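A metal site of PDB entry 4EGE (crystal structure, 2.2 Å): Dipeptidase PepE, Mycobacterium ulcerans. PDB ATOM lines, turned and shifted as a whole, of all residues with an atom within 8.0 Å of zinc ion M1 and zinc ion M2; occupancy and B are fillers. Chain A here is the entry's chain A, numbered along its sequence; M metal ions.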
ATOM      1  N   PHE A 204      25.322  25.777  -8.485  1.00  0.00           N
ATOM      2  CA  PHE A 204      26.610  25.215  -8.116  1.00  0.00           C
ATOM      3  C   PHE A 204      26.412  23.753  -7.779  1.00  0.00           C
ATOM      4  O   PHE A 204      25.330  23.357  -7.310  1.00  0.00           O
ATOM      5  CB  PHE A 204      27.192  25.938  -6.886  1.00  0.00           C
ATOM      6  CG  PHE A 204      26.254  25.926  -5.695  1.00  0.00           C
ATOM      7  CD1 PHE A 204      26.296  24.866  -4.773  1.00  0.00           C
ATOM      8  CD2 PHE A 204      25.325  26.944  -5.511  1.00  0.00           C
ATOM      9  CE1 PHE A 204      25.438  24.843  -3.681  1.00  0.00           C
ATOM     10  CE2 PHE A 204      24.458  26.923  -4.431  1.00  0.00           C
ATOM     11  CZ  PHE A 204      24.513  25.866  -3.519  1.00  0.00           C
ATOM     12  N   ILE A 206      28.742  20.767  -5.801  1.00  0.00           N
ATOM     13  CA  ILE A 206      29.938  20.357  -5.078  1.00  0.00           C
ATOM     14  C   ILE A 206      29.787  18.871  -4.765  1.00  0.00           C
ATOM     15  O   ILE A 206      28.788  18.466  -4.192  1.00  0.00           O
ATOM     16  CB  ILE A 206      30.132  21.205  -3.785  1.00  0.00           C
ATOM     17  CG1 ILE A 206      30.395  22.699  -4.109  1.00  0.00           C
ATOM     18  CG2 ILE A 206      31.262  20.623  -2.919  1.00  0.00           C
ATOM     19  CD1 ILE A 206      30.063  23.627  -2.949  1.00  0.00           C
ATOM     20  N   VAL A 233      27.837  16.438  -0.585  1.00  0.00           N
ATOM     21  CA  VAL A 233      27.112  16.904  -1.782  1.00  0.00           C
ATOM     22  C   VAL A 233      26.323  18.186  -1.454  1.00  0.00           C
ATOM     23  O   VAL A 233      25.352  18.158  -0.680  1.00  0.00           O
ATOM     24  CB  VAL A 233      26.201  15.822  -2.417  1.00  0.00           C
ATOM     25  CG1 VAL A 233      25.492  16.348  -3.658  1.00  0.00           C
ATOM     26  CG2 VAL A 233      27.004  14.570  -2.782  1.00  0.00           C
ATOM     27  N   ASP A 234      26.792  19.286  -2.035  1.00  0.00           N
ATOM     28  CA  ASP A 234      26.298  20.628  -1.751  1.00  0.00           C
ATOM     29  C   ASP A 234      25.884  21.202  -3.085  1.00  0.00           C
ATOM     30  O   ASP A 234      26.721  21.393  -3.959  1.00  0.00           O
ATOM     31  CB  ASP A 234      27.413  21.480  -1.135  1.00  0.00           C
ATOM     32  CG  ASP A 234      26.910  22.786  -0.545  1.00  0.00           C
ATOM     33  OD1 ASP A 234      25.738  23.168  -0.820  1.00  0.00           O
ATOM     34  OD2 ASP A 234      27.677  23.408   0.237  1.00  0.00           O
ATOM     35  N   ILE A 235      24.598  21.480  -3.245  1.00  0.00           N
ATOM     36  CA  ILE A 235      24.058  21.756  -4.562  1.00  0.00           C
ATOM     37  C   ILE A 235      22.947  22.788  -4.444  1.00  0.00           C
ATOM     38  O   ILE A 235      22.244  22.882  -3.389  1.00  0.00           O
ATOM     39  CB  ILE A 235      23.540  20.451  -5.247  1.00  0.00           C
ATOM     40  CG1 ILE A 235      22.546  19.711  -4.350  1.00  0.00           C
ATOM     41  CG2 ILE A 235      24.709  19.514  -5.613  1.00  0.00           C
ATOM     42  CD1 ILE A 235      21.762  18.612  -5.031  1.00  0.00           C
ATOM     43  N   GLY A 236      22.780  23.566  -5.517  1.00  0.00           N
ATOM     44  CA  GLY A 236      21.673  24.508  -5.593  1.00  0.00           C
ATOM     45  C   GLY A 236      21.380  24.926  -7.014  1.00  0.00           C
ATOM     46  O   GLY A 236      22.202  24.728  -7.931  1.00  0.00           O
ATOM     47  N   SER A 245      18.105  27.751  -4.154  1.00  0.00           N
ATOM     48  CA  SER A 245      18.146  26.595  -3.271  1.00  0.00           C
ATOM     49  C   SER A 245      19.631  26.379  -2.920  1.00  0.00           C
ATOM     50  O   SER A 245      20.529  26.881  -3.629  1.00  0.00           O
ATOM     51  CB  SER A 245      17.533  25.382  -3.957  1.00  0.00           C
ATOM     52  OG  SER A 245      18.302  25.037  -5.127  1.00  0.00           O
ATOM     53  N   ASP A 246      19.891  25.684  -1.804  1.00  0.00           N
ATOM     54  CA  ASP A 246      21.228  25.454  -1.297  1.00  0.00           C
ATOM     55  C   ASP A 246      21.124  24.457  -0.163  1.00  0.00           C
ATOM     56  O   ASP A 246      20.798  24.829   0.982  1.00  0.00           O
ATOM     57  CB  ASP A 246      21.873  26.763  -0.807  1.00  0.00           C
ATOM     58  CG  ASP A 246      23.304  26.583  -0.301  1.00  0.00           C
ATOM     59  OD1 ASP A 246      23.922  25.516  -0.566  1.00  0.00           O
ATOM     60  OD2 ASP A 246      23.821  27.511   0.369  1.00  0.00           O
ATOM     61  N   SER A 247      21.395  23.196  -0.487  1.00  0.00           N
ATOM     62  CA  SER A 247      21.327  22.118   0.501  1.00  0.00           C
ATOM     63  C   SER A 247      22.479  21.089   0.423  1.00  0.00           C
ATOM     64  O   SER A 247      22.831  20.602  -0.655  1.00  0.00           O
ATOM     65  CB  SER A 247      19.978  21.418   0.382  1.00  0.00           C
ATOM     66  OG  SER A 247      19.777  20.548   1.465  1.00  0.00           O
ATOM     67  N   THR A 248      23.045  20.732   1.574  1.00  0.00           N
ATOM     68  CA  THR A 248      24.137  19.744   1.620  1.00  0.00           C
ATOM     69  C   THR A 248      23.664  18.536   2.390  1.00  0.00           C
ATOM     70  O   THR A 248      23.042  18.675   3.445  1.00  0.00           O
ATOM     71  CB  THR A 248      25.402  20.302   2.315  1.00  0.00           C
ATOM     72  OG1 THR A 248      25.748  21.568   1.766  1.00  0.00           O
ATOM     73  CG2 THR A 248      26.579  19.378   2.161  1.00  0.00           C
ATOM     74  N   ARG A 249      23.987  17.342   1.877  1.00  0.00           N
ATOM     75  CA  ARG A 249      23.799  16.109   2.602  1.00  0.00           C
ATOM     76  C   ARG A 249      25.045  15.298   2.392  1.00  0.00           C
ATOM     77  O   ARG A 249      25.690  15.453   1.362  1.00  0.00           O
ATOM     78  CB  ARG A 249      22.566  15.343   2.110  1.00  0.00           C
ATOM     79  CG  ARG A 249      21.221  15.946   2.542  1.00  0.00           C
ATOM     80  CD  ARG A 249      21.092  15.994   4.060  1.00  0.00           C
ATOM     81  NE  ARG A 249      19.740  16.383   4.501  1.00  0.00           N
ATOM     82  CZ  ARG A 249      19.342  17.640   4.681  1.00  0.00           C
ATOM     83  NH1 ARG A 249      20.173  18.667   4.415  1.00  0.00           N
ATOM     84  NH2 ARG A 249      18.094  17.876   5.117  1.00  0.00           N
ATOM     85  N   ARG A 307      31.552  29.673   9.688  1.00  0.00           N
ATOM     86  CA  ARG A 307      30.283  30.105  10.222  1.00  0.00           C
ATOM     87  C   ARG A 307      29.171  29.049  10.022  1.00  0.00           C
ATOM     88  O   ARG A 307      29.276  28.161   9.170  1.00  0.00           O
ATOM     89  CB  ARG A 307      29.860  31.398   9.511  1.00  0.00           C
ATOM     90  CG  ARG A 307      29.585  31.200   8.027  1.00  0.00           C
ATOM     91  CD  ARG A 307      29.385  32.511   7.303  1.00  0.00           C
ATOM     92  NE  ARG A 307      29.098  32.268   5.891  1.00  0.00           N
ATOM     93  CZ  ARG A 307      29.320  33.130   4.902  1.00  0.00           C
ATOM     94  NH1 ARG A 307      29.817  34.332   5.149  1.00  0.00           N
ATOM     95  NH2 ARG A 307      29.019  32.773   3.640  1.00  0.00           N
ATOM     96  N   THR A 308      28.115  29.171  10.823  1.00  0.00           N
ATOM     97  CA  THR A 308      27.016  28.218  10.804  1.00  0.00           C
ATOM     98  C   THR A 308      26.117  28.418   9.586  1.00  0.00           C
ATOM     99  O   THR A 308      25.508  27.461   9.108  1.00  0.00           O
ATOM    100  CB  THR A 308      26.204  28.282  12.112  1.00  0.00           C
ATOM    101  OG1 THR A 308      26.996  27.732  13.154  1.00  0.00           O
ATOM    102  CG2 THR A 308      24.890  27.452  12.013  1.00  0.00           C
ATOM    103  N   GLY A 309      26.037  29.641   9.067  1.00  0.00           N
ATOM    104  CA  GLY A 309      25.161  29.889   7.910  1.00  0.00           C
ATOM    105  C   GLY A 309      25.176  31.289   7.320  1.00  0.00           C
ATOM    106  O   GLY A 309      25.759  32.203   7.900  1.00  0.00           O
ATOM    107  N   HIS A 310      24.498  31.442   6.185  1.00  0.00           N
ATOM    108  CA  HIS A 310      24.451  32.706   5.472  1.00  0.00           C
ATOM    109  C   HIS A 310      23.041  32.954   5.011  1.00  0.00           C
ATOM    110  O   HIS A 310      22.274  32.015   4.816  1.00  0.00           O
ATOM    111  CB  HIS A 310      25.369  32.631   4.249  1.00  0.00           C
ATOM    112  CG  HIS A 310      25.025  31.478   3.334  1.00  0.00           C
ATOM    113  ND1 HIS A 310      23.921  31.469   2.575  1.00  0.00           N
ATOM    114  CD2 HIS A 310      25.633  30.240   3.170  1.00  0.00           C
ATOM    115  CE1 HIS A 310      23.832  30.287   1.924  1.00  0.00           C
ATOM    116  NE2 HIS A 310      24.881  29.543   2.283  1.00  0.00           N
ATOM    117  N   GLY A 311      22.676  34.214   4.832  1.00  0.00           N
ATOM    118  CA  GLY A 311      21.379  34.538   4.272  1.00  0.00           C
ATOM    119  C   GLY A 311      21.309  34.069   2.830  1.00  0.00           C
ATOM    120  O   GLY A 311      22.325  33.820   2.172  1.00  0.00           O
ATOM    121  N   ILE A 312      20.099  33.929   2.326  1.00  0.00           N
ATOM    122  CA  ILE A 312      19.929  33.495   0.958  1.00  0.00           C
ATOM    123  C   ILE A 312      18.674  34.200   0.454  1.00  0.00           C
ATOM    124  O   ILE A 312      17.796  34.532   1.238  1.00  0.00           O
ATOM    125  CB  ILE A 312      19.849  31.934   0.878  1.00  0.00           C
ATOM    126  CG1 ILE A 312      19.845  31.436  -0.578  1.00  0.00           C
ATOM    127  CG2 ILE A 312      18.712  31.374   1.733  1.00  0.00           C
ATOM    128  CD1 ILE A 312      20.162  29.952  -0.686  1.00  0.00           C
ATOM    129  N   VAL A 316      23.022  33.578  -3.508  1.00  0.00           N
ATOM    130  CA  VAL A 316      23.271  32.398  -2.650  1.00  0.00           C
ATOM    131  C   VAL A 316      23.753  32.867  -1.259  1.00  0.00           C
ATOM    132  O   VAL A 316      23.466  32.232  -0.261  1.00  0.00           O
ATOM    133  CB  VAL A 316      24.289  31.402  -3.249  1.00  0.00           C
ATOM    134  CG1 VAL A 316      24.292  30.088  -2.494  1.00  0.00           C
ATOM    135  CG2 VAL A 316      23.954  31.085  -4.685  1.00  0.00           C
ATOM    136  N   HIS A 317      24.465  33.993  -1.209  1.00  0.00           N
ATOM    137  CA  HIS A 317      25.074  34.505   0.018  1.00  0.00           C
ATOM    138  C   HIS A 317      24.654  35.919   0.265  1.00  0.00           C
ATOM    139  O   HIS A 317      24.995  36.804  -0.513  1.00  0.00           O
ATOM    140  CB  HIS A 317      26.605  34.440  -0.097  1.00  0.00           C
ATOM    141  CG  HIS A 317      27.179  33.047   0.062  1.00  0.00           C
ATOM    142  ND1 HIS A 317      28.508  32.811   0.048  1.00  0.00           N
ATOM    143  CD2 HIS A 317      26.558  31.824   0.271  1.00  0.00           C
ATOM    144  CE1 HIS A 317      28.734  31.498   0.239  1.00  0.00           C
ATOM    145  NE2 HIS A 317      27.534  30.881   0.358  1.00  0.00           N
ATOM    146  N   PHE A 336      18.018  31.952   5.816  1.00  0.00           N
ATOM    147  CA  PHE A 336      19.445  31.679   5.862  1.00  0.00           C
ATOM    148  C   PHE A 336      19.647  30.171   5.975  1.00  0.00           C
ATOM    149  O   PHE A 336      18.711  29.417   6.291  1.00  0.00           O
ATOM    150  CB  PHE A 336      20.097  32.410   7.060  1.00  0.00           C
ATOM    151  CG  PHE A 336      19.324  32.288   8.348  1.00  0.00           C
ATOM    152  CD1 PHE A 336      19.456  31.155   9.155  1.00  0.00           C
ATOM    153  CD2 PHE A 336      18.445  33.291   8.741  1.00  0.00           C
ATOM    154  CE1 PHE A 336      18.757  31.035  10.340  1.00  0.00           C
ATOM    155  CE2 PHE A 336      17.709  33.183   9.914  1.00  0.00           C
ATOM    156  CZ  PHE A 336      17.872  32.048  10.720  1.00  0.00           C
ATOM    157  N   SER A 337      20.875  29.753   5.715  1.00  0.00           N
ATOM    158  CA  SER A 337      21.285  28.378   5.859  1.00  0.00           C
ATOM    159  C   SER A 337      21.686  28.077   7.305  1.00  0.00           C
ATOM    160  O   SER A 337      22.086  28.966   8.034  1.00  0.00           O
ATOM    161  CB  SER A 337      22.462  28.095   4.952  1.00  0.00           C
ATOM    162  OG  SER A 337      23.616  28.740   5.452  1.00  0.00           O
ATOM    163  N   ILE A 338      21.516  26.817   7.708  1.00  0.00           N
ATOM    164  CA  ILE A 338      22.130  26.285   8.900  1.00  0.00           C
ATOM    165  C   ILE A 338      22.958  25.116   8.371  1.00  0.00           C
ATOM    166  O   ILE A 338      22.386  24.139   7.867  1.00  0.00           O
ATOM    167  CB  ILE A 338      21.087  25.815   9.930  1.00  0.00           C
ATOM    168  CG1 ILE A 338      20.235  26.996  10.425  1.00  0.00           C
ATOM    169  CG2 ILE A 338      21.776  25.103  11.092  1.00  0.00           C
ATOM    170  CD1 ILE A 338      20.999  28.041  11.222  1.00  0.00           C
ATOM    171  N   GLU A 339      24.282  25.209   8.486  1.00  0.00           N
ATOM    172  CA  GLU A 339      25.184  24.283   7.799  1.00  0.00           C
ATOM    173  C   GLU A 339      26.505  24.031   8.517  1.00  0.00           C
ATOM    174  O   GLU A 339      27.593  24.247   7.946  1.00  0.00           O
ATOM    175  CB  GLU A 339      25.411  24.735   6.330  1.00  0.00           C
ATOM    176  CG  GLU A 339      25.869  26.184   6.150  1.00  0.00           C
ATOM    177  CD  GLU A 339      26.335  26.455   4.734  1.00  0.00           C
ATOM    178  OE1 GLU A 339      27.237  25.721   4.259  1.00  0.00           O
ATOM    179  OE2 GLU A 339      25.776  27.372   4.069  1.00  0.00           O
ATOM    180  N   ARG A 351      28.966  17.756   6.144  1.00  0.00           N
ATOM    181  CA  ARG A 351      28.230  18.979   6.352  1.00  0.00           C
ATOM    182  C   ARG A 351      26.736  18.678   6.182  1.00  0.00           C
ATOM    183  O   ARG A 351      26.337  17.902   5.324  1.00  0.00           O
ATOM    184  CB  ARG A 351      28.682  20.079   5.360  1.00  0.00           C
ATOM    185  CG  ARG A 351      28.047  21.443   5.639  1.00  0.00           C
ATOM    186  CD  ARG A 351      28.741  22.595   4.913  1.00  0.00           C
ATOM    187  NE  ARG A 351      28.727  22.494   3.447  1.00  0.00           N
ATOM    188  CZ  ARG A 351      29.756  22.090   2.712  1.00  0.00           C
ATOM    189  NH1 ARG A 351      30.904  21.745   3.297  1.00  0.00           N
ATOM    190  NH2 ARG A 351      29.651  22.037   1.390  1.00  0.00           N
ATOM    191  N   GLU A 353      23.234  20.724   5.651  1.00  0.00           N
ATOM    192  CA  GLU A 353      22.787  22.082   5.367  1.00  0.00           C
ATOM    193  C   GLU A 353      21.328  22.185   4.960  1.00  0.00           C
ATOM    194  O   GLU A 353      20.933  21.582   3.949  1.00  0.00           O
ATOM    195  CB  GLU A 353      23.655  22.733   4.295  1.00  0.00           C
ATOM    196  CG  GLU A 353      23.004  24.002   3.754  1.00  0.00           C
ATOM    197  CD  GLU A 353      23.890  24.785   2.805  1.00  0.00           C
ATOM    198  OE1 GLU A 353      24.693  24.150   2.061  1.00  0.00           O
ATOM    199  OE2 GLU A 353      23.769  26.029   2.835  1.00  0.00           O
ATOM    200  N   ASP A 354      20.567  22.962   5.723  1.00  0.00           N
ATOM    201  CA  ASP A 354      19.208  23.312   5.362  1.00  0.00           C
ATOM    202  C   ASP A 354      19.091  24.817   5.240  1.00  0.00           C
ATOM    203  O   ASP A 354      19.805  25.563   5.941  1.00  0.00           O
ATOM    204  CB  ASP A 354      18.220  22.885   6.433  1.00  0.00           C
ATOM    205  CG  ASP A 354      18.116  21.397   6.582  1.00  0.00           C
ATOM    206  OD1 ASP A 354      18.299  20.702   5.552  1.00  0.00           O
ATOM    207  OD2 ASP A 354      17.879  20.929   7.726  1.00  0.00           O
ATOM    208  N   ILE A 355      18.203  25.263   4.345  1.00  0.00           N
ATOM    209  CA  ILE A 355      17.711  26.632   4.366  1.00  0.00           C
ATOM    210  C   ILE A 355      16.470  26.678   5.235  1.00  0.00           C
ATOM    211  O   ILE A 355      15.538  25.871   5.040  1.00  0.00           O
ATOM    212  CB  ILE A 355      17.314  27.148   2.953  1.00  0.00           C
ATOM    213  CG1 ILE A 355      18.514  27.141   1.992  1.00  0.00           C
ATOM    214  CG2 ILE A 355      16.617  28.507   3.058  1.00  0.00           C
ATOM    215  CD1 ILE A 355      19.795  27.695   2.606  1.00  0.00           C
HETATM  216 ZN    ZN M   1      25.058  27.474   1.971  1.00  0.00          ZN
HETATM  217 ZN    ZN M   2      25.580  24.949   0.328  1.00  0.00          ZN
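O of His 310 sits at hydrogen-bond distance from N of Ser 337 (2.8 Å). N of Glu 353 is in hydrogen-bond range of O of Thr 248 (3.0 Å). O of Glu 353 sits at hydrogen-bond distance from OG of Ser 247, 2.9 Å away. NH1 of Arg 249 is in hydrogen-bond range of O of Glu 353 (3.0 Å). The guanidinium group (NH2) of Arg 351 is in salt-bridge range of the side-chain carboxylate (OD2) of Asp 234, at 2.7 Å. The backbone NH (N) of Ile 206 lies within hydrogen-bond range of the backbone carbonyl oxygen (O) of Asp 234, at 2.8 Å. The side-chain carboxylate (OE2) of Glu 339 lies close to the side-chain hydroxyl (OG) of Ser 337 (2.9 Å). The backbone carbonyl oxygen of Thr 308 sits at hydrogen-bond distance from the backbone NH of Glu 339, 2.6 Å away.
Residues that only touch zinc ion M1: Ser 337 (3.97 Å).
Merely in contact with zinc ion M2: Thr 248. Four residues have an atom within 4 Å of zinc ion M2: Asp 234, Asp 246, Thr 248 and Glu 353.
Zinc ion M1 is bound by OD2 of Asp 246 (2.0 Å), NE2 of His 310 (2.1 Å), OE2 of Glu 353 (2.1 Å) and OE2 of Glu 339 (2.2 Å). Zinc ion M1 has four donor atoms within binding distance.
Zinc ion M2 is bound by OD1 of Asp 246 (2.0 Å), OE1 of Glu 353 (2.1 Å) and OD1 of Asp 234 (2.1 Å). Zinc ion M2 has three donor atoms within binding distance. Slightly farther from zinc ion M2 lies the side-chain carboxylate (OD2) of Asp 234 (2.6 Å).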
